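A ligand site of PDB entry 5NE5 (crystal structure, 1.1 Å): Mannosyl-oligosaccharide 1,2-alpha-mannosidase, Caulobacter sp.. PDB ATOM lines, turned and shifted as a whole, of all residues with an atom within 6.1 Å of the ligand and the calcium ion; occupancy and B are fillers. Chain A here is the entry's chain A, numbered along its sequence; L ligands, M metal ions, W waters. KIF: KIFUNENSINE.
The calcium ion is bound by water W5. Water W2 binds the calcium ion (2.4 Å). The calcium ion is bound by water W3, 2.5 Å away. O of Thr 428 binds the calcium ion. The calcium ion is bound by an oxygen (O2) of the ligand (2.5 Å). The calcium ion is bound by OG1 of Thr 428 (2.5 Å). O3 of the ligand is bound to the calcium ion, 2.5 Å away. Water W9 binds the calcium ion (2.6 Å).
OE1 of Glu 342 sits close to OE1 of Glu 286. The guanidinium group (NH1) of Arg 340 sits at hydrogen-bond distance from the side-chain hydroxyl (OH) of Tyr 400, 3.2 Å away. The backbone NH (N) of Glu 429 lies within hydrogen-bond range of the side-chain hydroxyl (OG) of Ser 427. The guanidinium group (NH1) of Arg 102 is in salt-bridge range of the side-chain carboxylate (OE2) of Glu 429. The backbone carbonyl oxygen (O) of Gly 338 sits at hydrogen-bond distance from the side-chain hydroxyl (OH) of Tyr 400, 2.6 Å away. The side-chain hydroxyl (OH) of Tyr 408 is in hydrogen-bond range of the side-chain carboxylate (OE1) of Glu 404 (2.6 Å). The side-chain hydroxyl (OG1) of Thr 428 lies close to the side-chain carboxylate (OE1) of Glu 230, at 2.6 Å. The side-chain hydroxyl (OH) of Tyr 290 lies within hydrogen-bond range of the backbone carbonyl oxygen (O) of Asp 226, 3.2 Å away.
Water W2 bridges the side-chain carboxylate of Asp 345 and the side-chain carboxylate of Glu 230. Water W3 bridges the side-chain carboxylate (OE1) of Glu 404 and the side-chain carboxylate (OD2) of Asp 345. Water W6 lies within hydrogen-bond range of the side-chain hydroxyl of Ser 227 (2.7 Å), the side-chain carboxylate of Asp 226 (2.8 Å) and a nitrogen (N9) of the ligand (3.2 Å). Water W8 bridges an oxygen (O8) of the ligand (2.8 Å) and the side-chain carboxylate of Asp 226 (2.8 Å). Water W4 lies within hydrogen-bond range of an oxygen (O4) of the ligand (2.8 Å) and the side-chain carboxylate (OE1) of Glu 98 (2.9 Å). Water W7 lies within hydrogen-bond range of NH2 of Arg 340 (2.9 Å) and O7 of the ligand (3.0 Å).
Ile 101 touches the ligand. Leu 287 touches the ligand. CD of Pro 341 touches O6 of the ligand, 3.6 Å away. Tyr 400 touches the ligand. Hydrophobic or aromatic side chains that line the ligand: Ile 101, Leu 287, Pro 341 and Tyr 400.
The guanidinium group (NH1) of Arg 340 is in hydrogen-bond range of an oxygen (O6) of the ligand. N9 of the ligand is in hydrogen-bond range of OD2 of Asp 226. O3 of the ligand lies close to OE2 of Glu 404, at 2.6 Å. OE2 of Glu 342 is in hydrogen-bond range of O6 of the ligand (2.7 Å). OE1 of Glu 429 is in hydrogen-bond range of O4 of the ligand.
Of the 21 residues printed, 1 comes within 4 Å of the calcium ion.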
ATOM      1  N   PHE A  97     -22.892 -27.016  35.897  1.00  0.00           N
ATOM      2  CA  PHE A  97     -22.343 -26.098  34.881  1.00  0.00           C
ATOM      3  C   PHE A  97     -23.158 -24.820  34.789  1.00  0.00           C
ATOM      4  O   PHE A  97     -22.644 -23.670  34.816  1.00  0.00           O
ATOM      5  CB  PHE A  97     -22.234 -26.854  33.530  1.00  0.00           C
ATOM      6  CG  PHE A  97     -22.014 -25.961  32.322  1.00  0.00           C
ATOM      7  CD1 PHE A  97     -20.734 -25.549  31.941  1.00  0.00           C
ATOM      8  CD2 PHE A  97     -23.098 -25.646  31.516  1.00  0.00           C
ATOM      9  CE1 PHE A  97     -20.572 -24.763  30.770  1.00  0.00           C
ATOM     10  CE2 PHE A  97     -22.950 -24.849  30.386  1.00  0.00           C
ATOM     11  CZ  PHE A  97     -21.674 -24.416  30.008  1.00  0.00           C
ATOM     12  N   GLU A  98     -24.487 -24.998  34.549  1.00  0.00           N
ATOM     13  CA  GLU A  98     -25.380 -23.826  34.343  1.00  0.00           C
ATOM     14  C   GLU A  98     -25.414 -22.950  35.637  1.00  0.00           C
ATOM     15  O   GLU A  98     -25.435 -21.710  35.572  1.00  0.00           O
ATOM     16  CB  GLU A  98     -26.801 -24.309  34.018  1.00  0.00           C
ATOM     17  CG  GLU A  98     -26.942 -25.152  32.712  1.00  0.00           C
ATOM     18  CD  GLU A  98     -26.688 -24.436  31.425  1.00  0.00           C
ATOM     19  OE1 GLU A  98     -26.499 -23.172  31.374  1.00  0.00           O
ATOM     20  OE2 GLU A  98     -26.688 -25.166  30.353  1.00  0.00           O
ATOM     21  N   ILE A 101     -22.026 -20.859  35.885  1.00  0.00           N
ATOM     22  CA  ILE A 101     -21.751 -19.750  34.947  1.00  0.00           C
ATOM     23  C   ILE A 101     -22.795 -18.640  35.069  1.00  0.00           C
ATOM     24  O   ILE A 101     -22.508 -17.466  34.811  1.00  0.00           O
ATOM     25  CB  ILE A 101     -21.522 -20.227  33.485  1.00  0.00           C
ATOM     26  CG1 ILE A 101     -22.807 -20.756  32.799  1.00  0.00           C
ATOM     27  CG2 ILE A 101     -20.370 -21.224  33.432  1.00  0.00           C
ATOM     28  CD1 ILE A 101     -22.622 -21.091  31.342  1.00  0.00           C
ATOM     29  N   ARG A 102     -24.040 -19.013  35.412  1.00  0.00           N
ATOM     30  CA  ARG A 102     -25.159 -18.038  35.477  1.00  0.00           C
ATOM     31  C   ARG A 102     -25.304 -17.382  36.871  1.00  0.00           C
ATOM     32  O   ARG A 102     -25.394 -16.147  36.974  1.00  0.00           O
ATOM     33  CB  ARG A 102     -26.485 -18.718  35.070  1.00  0.00           C
ATOM     34  CG  ARG A 102     -26.481 -19.265  33.654  1.00  0.00           C
ATOM     35  CD  ARG A 102     -27.720 -20.073  33.339  1.00  0.00           C
ATOM     36  NE  ARG A 102     -27.715 -20.707  32.000  1.00  0.00           N
ATOM     37  CZ  ARG A 102     -28.478 -20.321  30.979  1.00  0.00           C
ATOM     38  NH1 ARG A 102     -29.141 -19.152  31.010  1.00  0.00           N
ATOM     39  NH2 ARG A 102     -28.567 -21.122  29.902  1.00  0.00           N
ATOM     40  N   ASP A 226     -16.804 -26.017  24.002  1.00  0.00           N
ATOM     41  CA  ASP A 226     -16.513 -24.615  23.752  1.00  0.00           C
ATOM     42  C   ASP A 226     -15.700 -23.934  24.861  1.00  0.00           C
ATOM     43  O   ASP A 226     -14.534 -23.503  24.636  1.00  0.00           O
ATOM     44  CB  ASP A 226     -17.810 -23.833  23.384  1.00  0.00           C
ATOM     45  CG  ASP A 226     -19.025 -23.920  24.345  1.00  0.00           C
ATOM     46  OD1 ASP A 226     -18.973 -24.573  25.419  1.00  0.00           O
ATOM     47  OD2 ASP A 226     -20.067 -23.305  24.002  1.00  0.00           O
ATOM     48  N   SER A 227     -16.310 -23.711  26.043  1.00  0.00           N
ATOM     49  CA  SER A 227     -15.708 -22.827  27.038  1.00  0.00           C
ATOM     50  C   SER A 227     -14.497 -23.409  27.791  1.00  0.00           C
ATOM     51  O   SER A 227     -13.804 -22.672  28.506  1.00  0.00           O
ATOM     52  CB  SER A 227     -16.780 -22.312  28.012  1.00  0.00           C
ATOM     53  OG  SER A 227     -17.597 -23.372  28.483  1.00  0.00           O
ATOM     54  N   GLU A 230     -11.581 -21.532  26.269  1.00  0.00           N
ATOM     55  CA  GLU A 230     -11.672 -20.121  26.703  1.00  0.00           C
ATOM     56  C   GLU A 230     -11.070 -19.978  28.147  1.00  0.00           C
ATOM     57  O   GLU A 230     -10.278 -19.046  28.449  1.00  0.00           O
ATOM     58  CB  GLU A 230     -13.173 -19.783  26.628  1.00  0.00           C
ATOM     59  CG  GLU A 230     -13.618 -18.416  26.910  1.00  0.00           C
ATOM     60  CD  GLU A 230     -15.145 -18.257  26.846  1.00  0.00           C
ATOM     61  OE1 GLU A 230     -15.875 -19.285  26.716  1.00  0.00           O
ATOM     62  OE2 GLU A 230     -15.628 -17.072  26.979  1.00  0.00           O
ATOM     63  N   GLU A 286     -23.695 -22.583  15.581  1.00  0.00           N
ATOM     64  CA  GLU A 286     -23.540 -21.125  15.778  1.00  0.00           C
ATOM     65  C   GLU A 286     -22.655 -20.827  16.982  1.00  0.00           C
ATOM     66  O   GLU A 286     -21.939 -19.771  16.997  1.00  0.00           O
ATOM     67  CB  GLU A 286     -24.926 -20.457  15.919  1.00  0.00           C
ATOM     68  CG  GLU A 286     -24.931 -18.926  16.015  1.00  0.00           C
ATOM     69  CD  GLU A 286     -24.487 -18.356  17.362  1.00  0.00           C
ATOM     70  OE1 GLU A 286     -24.542 -19.169  18.385  1.00  0.00           O
ATOM     71  OE2 GLU A 286     -24.111 -17.161  17.453  1.00  0.00           O
ATOM     72  N   LEU A 287     -22.688 -21.686  18.000  1.00  0.00           N
ATOM     73  CA  LEU A 287     -21.866 -21.530  19.265  1.00  0.00           C
ATOM     74  C   LEU A 287     -20.422 -21.360  18.977  1.00  0.00           C
ATOM     75  O   LEU A 287     -19.656 -20.800  19.786  1.00  0.00           O
ATOM     76  CB  LEU A 287     -21.934 -22.785  20.246  1.00  0.00           C
ATOM     77  CG  LEU A 287     -23.268 -23.091  20.887  1.00  0.00           C
ATOM     78  CD1 LEU A 287     -23.205 -24.405  21.684  1.00  0.00           C
ATOM     79  CD2 LEU A 287     -23.738 -21.921  21.762  1.00  0.00           C
ATOM     80  N   TYR A 290     -17.760 -17.922  19.038  1.00  0.00           N
ATOM     81  CA  TYR A 290     -16.879 -17.462  20.178  1.00  0.00           C
ATOM     82  C   TYR A 290     -15.415 -17.613  19.808  1.00  0.00           C
ATOM     83  O   TYR A 290     -14.542 -16.797  20.249  1.00  0.00           O
ATOM     84  CB  TYR A 290     -17.126 -18.274  21.551  1.00  0.00           C
ATOM     85  CG  TYR A 290     -16.373 -19.596  21.638  1.00  0.00           C
ATOM     86  CD1 TYR A 290     -16.810 -20.730  20.978  1.00  0.00           C
ATOM     87  CD2 TYR A 290     -15.167 -19.666  22.317  1.00  0.00           C
ATOM     88  CE1 TYR A 290     -16.097 -21.898  20.939  1.00  0.00           C
ATOM     89  CE2 TYR A 290     -14.378 -20.852  22.245  1.00  0.00           C
ATOM     90  CZ  TYR A 290     -14.854 -21.971  21.582  1.00  0.00           C
ATOM     91  OH  TYR A 290     -14.095 -23.062  21.547  1.00  0.00           O
ATOM     92  N   GLY A 338     -31.808 -20.020  19.216  1.00  0.00           N
ATOM     93  CA  GLY A 338     -31.757 -19.741  20.624  1.00  0.00           C
ATOM     94  C   GLY A 338     -31.478 -18.244  20.947  1.00  0.00           C
ATOM     95  O   GLY A 338     -30.966 -17.975  22.047  1.00  0.00           O
ATOM     96  N   ARG A 340     -29.093 -16.172  19.961  1.00  0.00           N
ATOM     97  CA  ARG A 340     -27.723 -16.485  20.394  1.00  0.00           C
ATOM     98  C   ARG A 340     -26.774 -15.294  20.377  1.00  0.00           C
ATOM     99  O   ARG A 340     -26.796 -14.467  19.417  1.00  0.00           O
ATOM    100  CB  ARG A 340     -27.115 -17.628  19.548  1.00  0.00           C
ATOM    101  CG  ARG A 340     -27.834 -18.992  19.729  1.00  0.00           C
ATOM    102  CD  ARG A 340     -27.510 -19.660  21.056  1.00  0.00           C
ATOM    103  NE  ARG A 340     -28.278 -20.918  21.222  1.00  0.00           N
ATOM    104  CZ  ARG A 340     -28.213 -21.727  22.294  1.00  0.00           C
ATOM    105  NH1 ARG A 340     -27.450 -21.411  23.308  1.00  0.00           N
ATOM    106  NH2 ARG A 340     -28.992 -22.825  22.331  1.00  0.00           N
ATOM    107  N   PRO A 341     -25.801 -15.217  21.339  1.00  0.00           N
ATOM    108  CA  PRO A 341     -24.948 -14.027  21.490  1.00  0.00           C
ATOM    109  C   PRO A 341     -23.516 -14.172  20.937  1.00  0.00           C
ATOM    110  O   PRO A 341     -22.710 -13.211  21.095  1.00  0.00           O
ATOM    111  CB  PRO A 341     -24.840 -13.885  23.020  1.00  0.00           C
ATOM    112  CG  PRO A 341     -24.819 -15.328  23.484  1.00  0.00           C
ATOM    113  CD  PRO A 341     -25.841 -16.039  22.617  1.00  0.00           C
ATOM    114  N   GLU A 342     -23.127 -15.323  20.327  1.00  0.00           N
ATOM    115  CA  GLU A 342     -21.677 -15.560  20.077  1.00  0.00           C
ATOM    116  C   GLU A 342     -21.062 -14.632  19.007  1.00  0.00           C
ATOM    117  O   GLU A 342     -19.823 -14.405  19.079  1.00  0.00           O
ATOM    118  CB  GLU A 342     -21.397 -17.030  19.783  1.00  0.00           C
ATOM    119  CG  GLU A 342     -21.520 -17.941  21.024  1.00  0.00           C
ATOM    120  CD  GLU A 342     -22.968 -18.275  21.455  1.00  0.00           C
ATOM    121  OE1 GLU A 342     -23.935 -18.094  20.641  1.00  0.00           O
ATOM    122  OE2 GLU A 342     -23.095 -18.769  22.613  1.00  0.00           O
ATOM    123  N   ASP A 345     -20.117 -11.407  20.728  1.00  0.00           N
ATOM    124  CA  ASP A 345     -19.022 -11.830  21.659  1.00  0.00           C
ATOM    125  C   ASP A 345     -17.676 -11.706  20.905  1.00  0.00           C
ATOM    126  O   ASP A 345     -16.724 -11.036  21.348  1.00  0.00           O
ATOM    127  CB  ASP A 345     -19.328 -13.269  22.111  1.00  0.00           C
ATOM    128  CG  ASP A 345     -18.260 -13.937  22.987  1.00  0.00           C
ATOM    129  OD1 ASP A 345     -17.109 -13.473  23.045  1.00  0.00           O
ATOM    130  OD2 ASP A 345     -18.630 -14.999  23.605  1.00  0.00           O
ATOM    131  N   TYR A 400     -29.409 -15.989  29.310  1.00  0.00           N
ATOM    132  CA  TYR A 400     -28.126 -15.414  28.872  1.00  0.00           C
ATOM    133  C   TYR A 400     -28.302 -14.097  28.061  1.00  0.00           C
ATOM    134  O   TYR A 400     -27.370 -13.279  28.031  1.00  0.00           O
ATOM    135  CB  TYR A 400     -27.257 -16.428  28.081  1.00  0.00           C
ATOM    136  CG  TYR A 400     -27.975 -17.189  26.953  1.00  0.00           C
ATOM    137  CD1 TYR A 400     -28.340 -16.596  25.730  1.00  0.00           C
ATOM    138  CD2 TYR A 400     -28.238 -18.569  27.088  1.00  0.00           C
ATOM    139  CE1 TYR A 400     -28.948 -17.333  24.689  1.00  0.00           C
ATOM    140  CE2 TYR A 400     -28.867 -19.295  26.081  1.00  0.00           C
ATOM    141  CZ  TYR A 400     -29.225 -18.696  24.893  1.00  0.00           C
ATOM    142  OH  TYR A 400     -29.892 -19.427  23.938  1.00  0.00           O
ATOM    143  N   GLU A 404     -25.460 -11.143  28.159  1.00  0.00           N
ATOM    144  CA  GLU A 404     -24.546 -11.189  26.999  1.00  0.00           C
ATOM    145  C   GLU A 404     -24.774 -10.116  25.931  1.00  0.00           C
ATOM    146  O   GLU A 404     -24.057  -9.097  25.918  1.00  0.00           O
ATOM    147  CB  GLU A 404     -24.483 -12.622  26.396  1.00  0.00           C
ATOM    148  CG  GLU A 404     -24.016 -13.680  27.407  1.00  0.00           C
ATOM    149  CD  GLU A 404     -23.311 -14.874  26.766  1.00  0.00           C
ATOM    150  OE1 GLU A 404     -22.452 -14.623  25.839  1.00  0.00           O
ATOM    151  OE2 GLU A 404     -23.622 -16.001  27.173  1.00  0.00           O
ATOM    152  N   TYR A 408     -22.644  -6.699  25.207  1.00  0.00           N
ATOM    153  CA  TYR A 408     -21.641  -6.605  24.131  1.00  0.00           C
ATOM    154  C   TYR A 408     -21.869  -5.361  23.236  1.00  0.00           C
ATOM    155  O   TYR A 408     -20.926  -4.601  22.943  1.00  0.00           O
ATOM    156  CB  TYR A 408     -21.580  -7.889  23.265  1.00  0.00           C
ATOM    157  CG  TYR A 408     -21.265  -9.199  23.964  1.00  0.00           C
ATOM    158  CD1 TYR A 408     -20.367  -9.285  25.026  1.00  0.00           C
ATOM    159  CD2 TYR A 408     -21.870 -10.380  23.547  1.00  0.00           C
ATOM    160  CE1 TYR A 408     -20.110 -10.507  25.663  1.00  0.00           C
ATOM    161  CE2 TYR A 408     -21.644 -11.621  24.174  1.00  0.00           C
ATOM    162  CZ  TYR A 408     -20.748 -11.672  25.251  1.00  0.00           C
ATOM    163  OH  TYR A 408     -20.509 -12.868  25.904  1.00  0.00           O
ATOM    164  N   SER A 427     -16.483 -13.319  31.758  1.00  0.00           N
ATOM    165  CA  SER A 427     -16.664 -14.782  31.801  1.00  0.00           C
ATOM    166  C   SER A 427     -17.317 -15.310  30.506  1.00  0.00           C
ATOM    167  O   SER A 427     -17.680 -14.509  29.622  1.00  0.00           O
ATOM    168  CB  SER A 427     -17.534 -15.172  33.033  1.00  0.00           C
ATOM    169  OG  SER A 427     -18.922 -15.027  32.716  1.00  0.00           O
ATOM    170  N   THR A 428     -17.520 -16.643  30.421  1.00  0.00           N
ATOM    171  CA  THR A 428     -18.180 -17.163  29.204  1.00  0.00           C
ATOM    172  C   THR A 428     -19.670 -16.754  29.084  1.00  0.00           C
ATOM    173  O   THR A 428     -20.282 -16.919  28.007  1.00  0.00           O
ATOM    174  CB  THR A 428     -18.022 -18.722  29.083  1.00  0.00           C
ATOM    175  OG1 THR A 428     -18.250 -19.083  27.702  1.00  0.00           O
ATOM    176  CG2 THR A 428     -18.989 -19.483  29.969  1.00  0.00           C
ATOM    177  N   GLU A 429     -20.247 -16.305  30.232  1.00  0.00           N
ATOM    178  CA  GLU A 429     -21.620 -15.803  30.330  1.00  0.00           C
ATOM    179  C   GLU A 429     -21.640 -14.246  30.298  1.00  0.00           C
ATOM    180  O   GLU A 429     -22.654 -13.608  30.593  1.00  0.00           O
ATOM    181  CB  GLU A 429     -22.246 -16.319  31.666  1.00  0.00           C
ATOM    182  CG  GLU A 429     -23.765 -16.182  31.794  1.00  0.00           C
ATOM    183  CD  GLU A 429     -24.565 -17.183  30.979  1.00  0.00           C
ATOM    184  OE1 GLU A 429     -24.013 -18.096  30.344  1.00  0.00           O
ATOM    185  OE2 GLU A 429     -25.868 -17.055  30.976  1.00  0.00           O
HETATM  186  C4  KIF L   1     -24.493 -19.217  27.395  1.00  0.00           C
HETATM  187  O4  KIF L   1     -24.981 -19.941  28.535  1.00  0.00           O
HETATM  188  C3  KIF L   1     -22.945 -19.179  27.424  1.00  0.00           C
HETATM  189  O3  KIF L   1     -22.409 -18.247  26.463  1.00  0.00           O
HETATM  190  C2  KIF L   1     -22.321 -20.556  27.077  1.00  0.00           C
HETATM  191  O2  KIF L   1     -20.895 -20.381  27.034  1.00  0.00           O
HETATM  192  C1  KIF L   1     -22.864 -21.020  25.723  1.00  0.00           C
HETATM  193  N9  KIF L   1     -22.510 -22.436  25.395  1.00  0.00           N
HETATM  194  C8  KIF L   1     -23.609 -23.184  25.303  1.00  0.00           C
HETATM  195  O8  KIF L   1     -23.630 -24.410  25.070  1.00  0.00           O
HETATM  196  C7  KIF L   1     -24.814 -22.337  25.578  1.00  0.00           C
HETATM  197  O7  KIF L   1     -25.992 -22.686  25.553  1.00  0.00           O
HETATM  198  N   KIF L   1     -24.323 -21.076  25.762  1.00  0.00           N
HETATM  199  C5  KIF L   1     -25.074 -19.844  26.120  1.00  0.00           C
HETATM  200  C6  KIF L   1     -25.118 -18.837  24.970  1.00  0.00           C
HETATM  201  O6  KIF L   1     -25.437 -19.429  23.699  1.00  0.00           O
HETATM  202 CA    CA M   1     -19.932 -18.321  25.990  1.00  0.00          CA
HETATM  203  O   HOH W   1     -26.087 -25.400  23.906  1.00  0.00           O
HETATM  204  O   HOH W   2     -18.013 -16.890  25.546  1.00  0.00           O
HETATM  205  O   HOH W   3     -20.821 -16.400  24.718  1.00  0.00           O
HETATM  206  O   HOH W   4     -25.529 -22.706  28.713  1.00  0.00           O
HETATM  207  O   HOH W   5     -20.789 -19.214  23.973  1.00  0.00           O
HETATM  208  O   HOH W   6     -20.056 -22.907  27.446  1.00  0.00           O
HETATM  209  O   HOH W   7     -28.406 -24.272  24.814  1.00  0.00           O
HETATM  210  O   HOH W   8     -21.410 -26.011  25.574  1.00  0.00           O
HETATM  211  O   HOH W   9     -18.248 -20.005  24.993  1.00  0.00           O
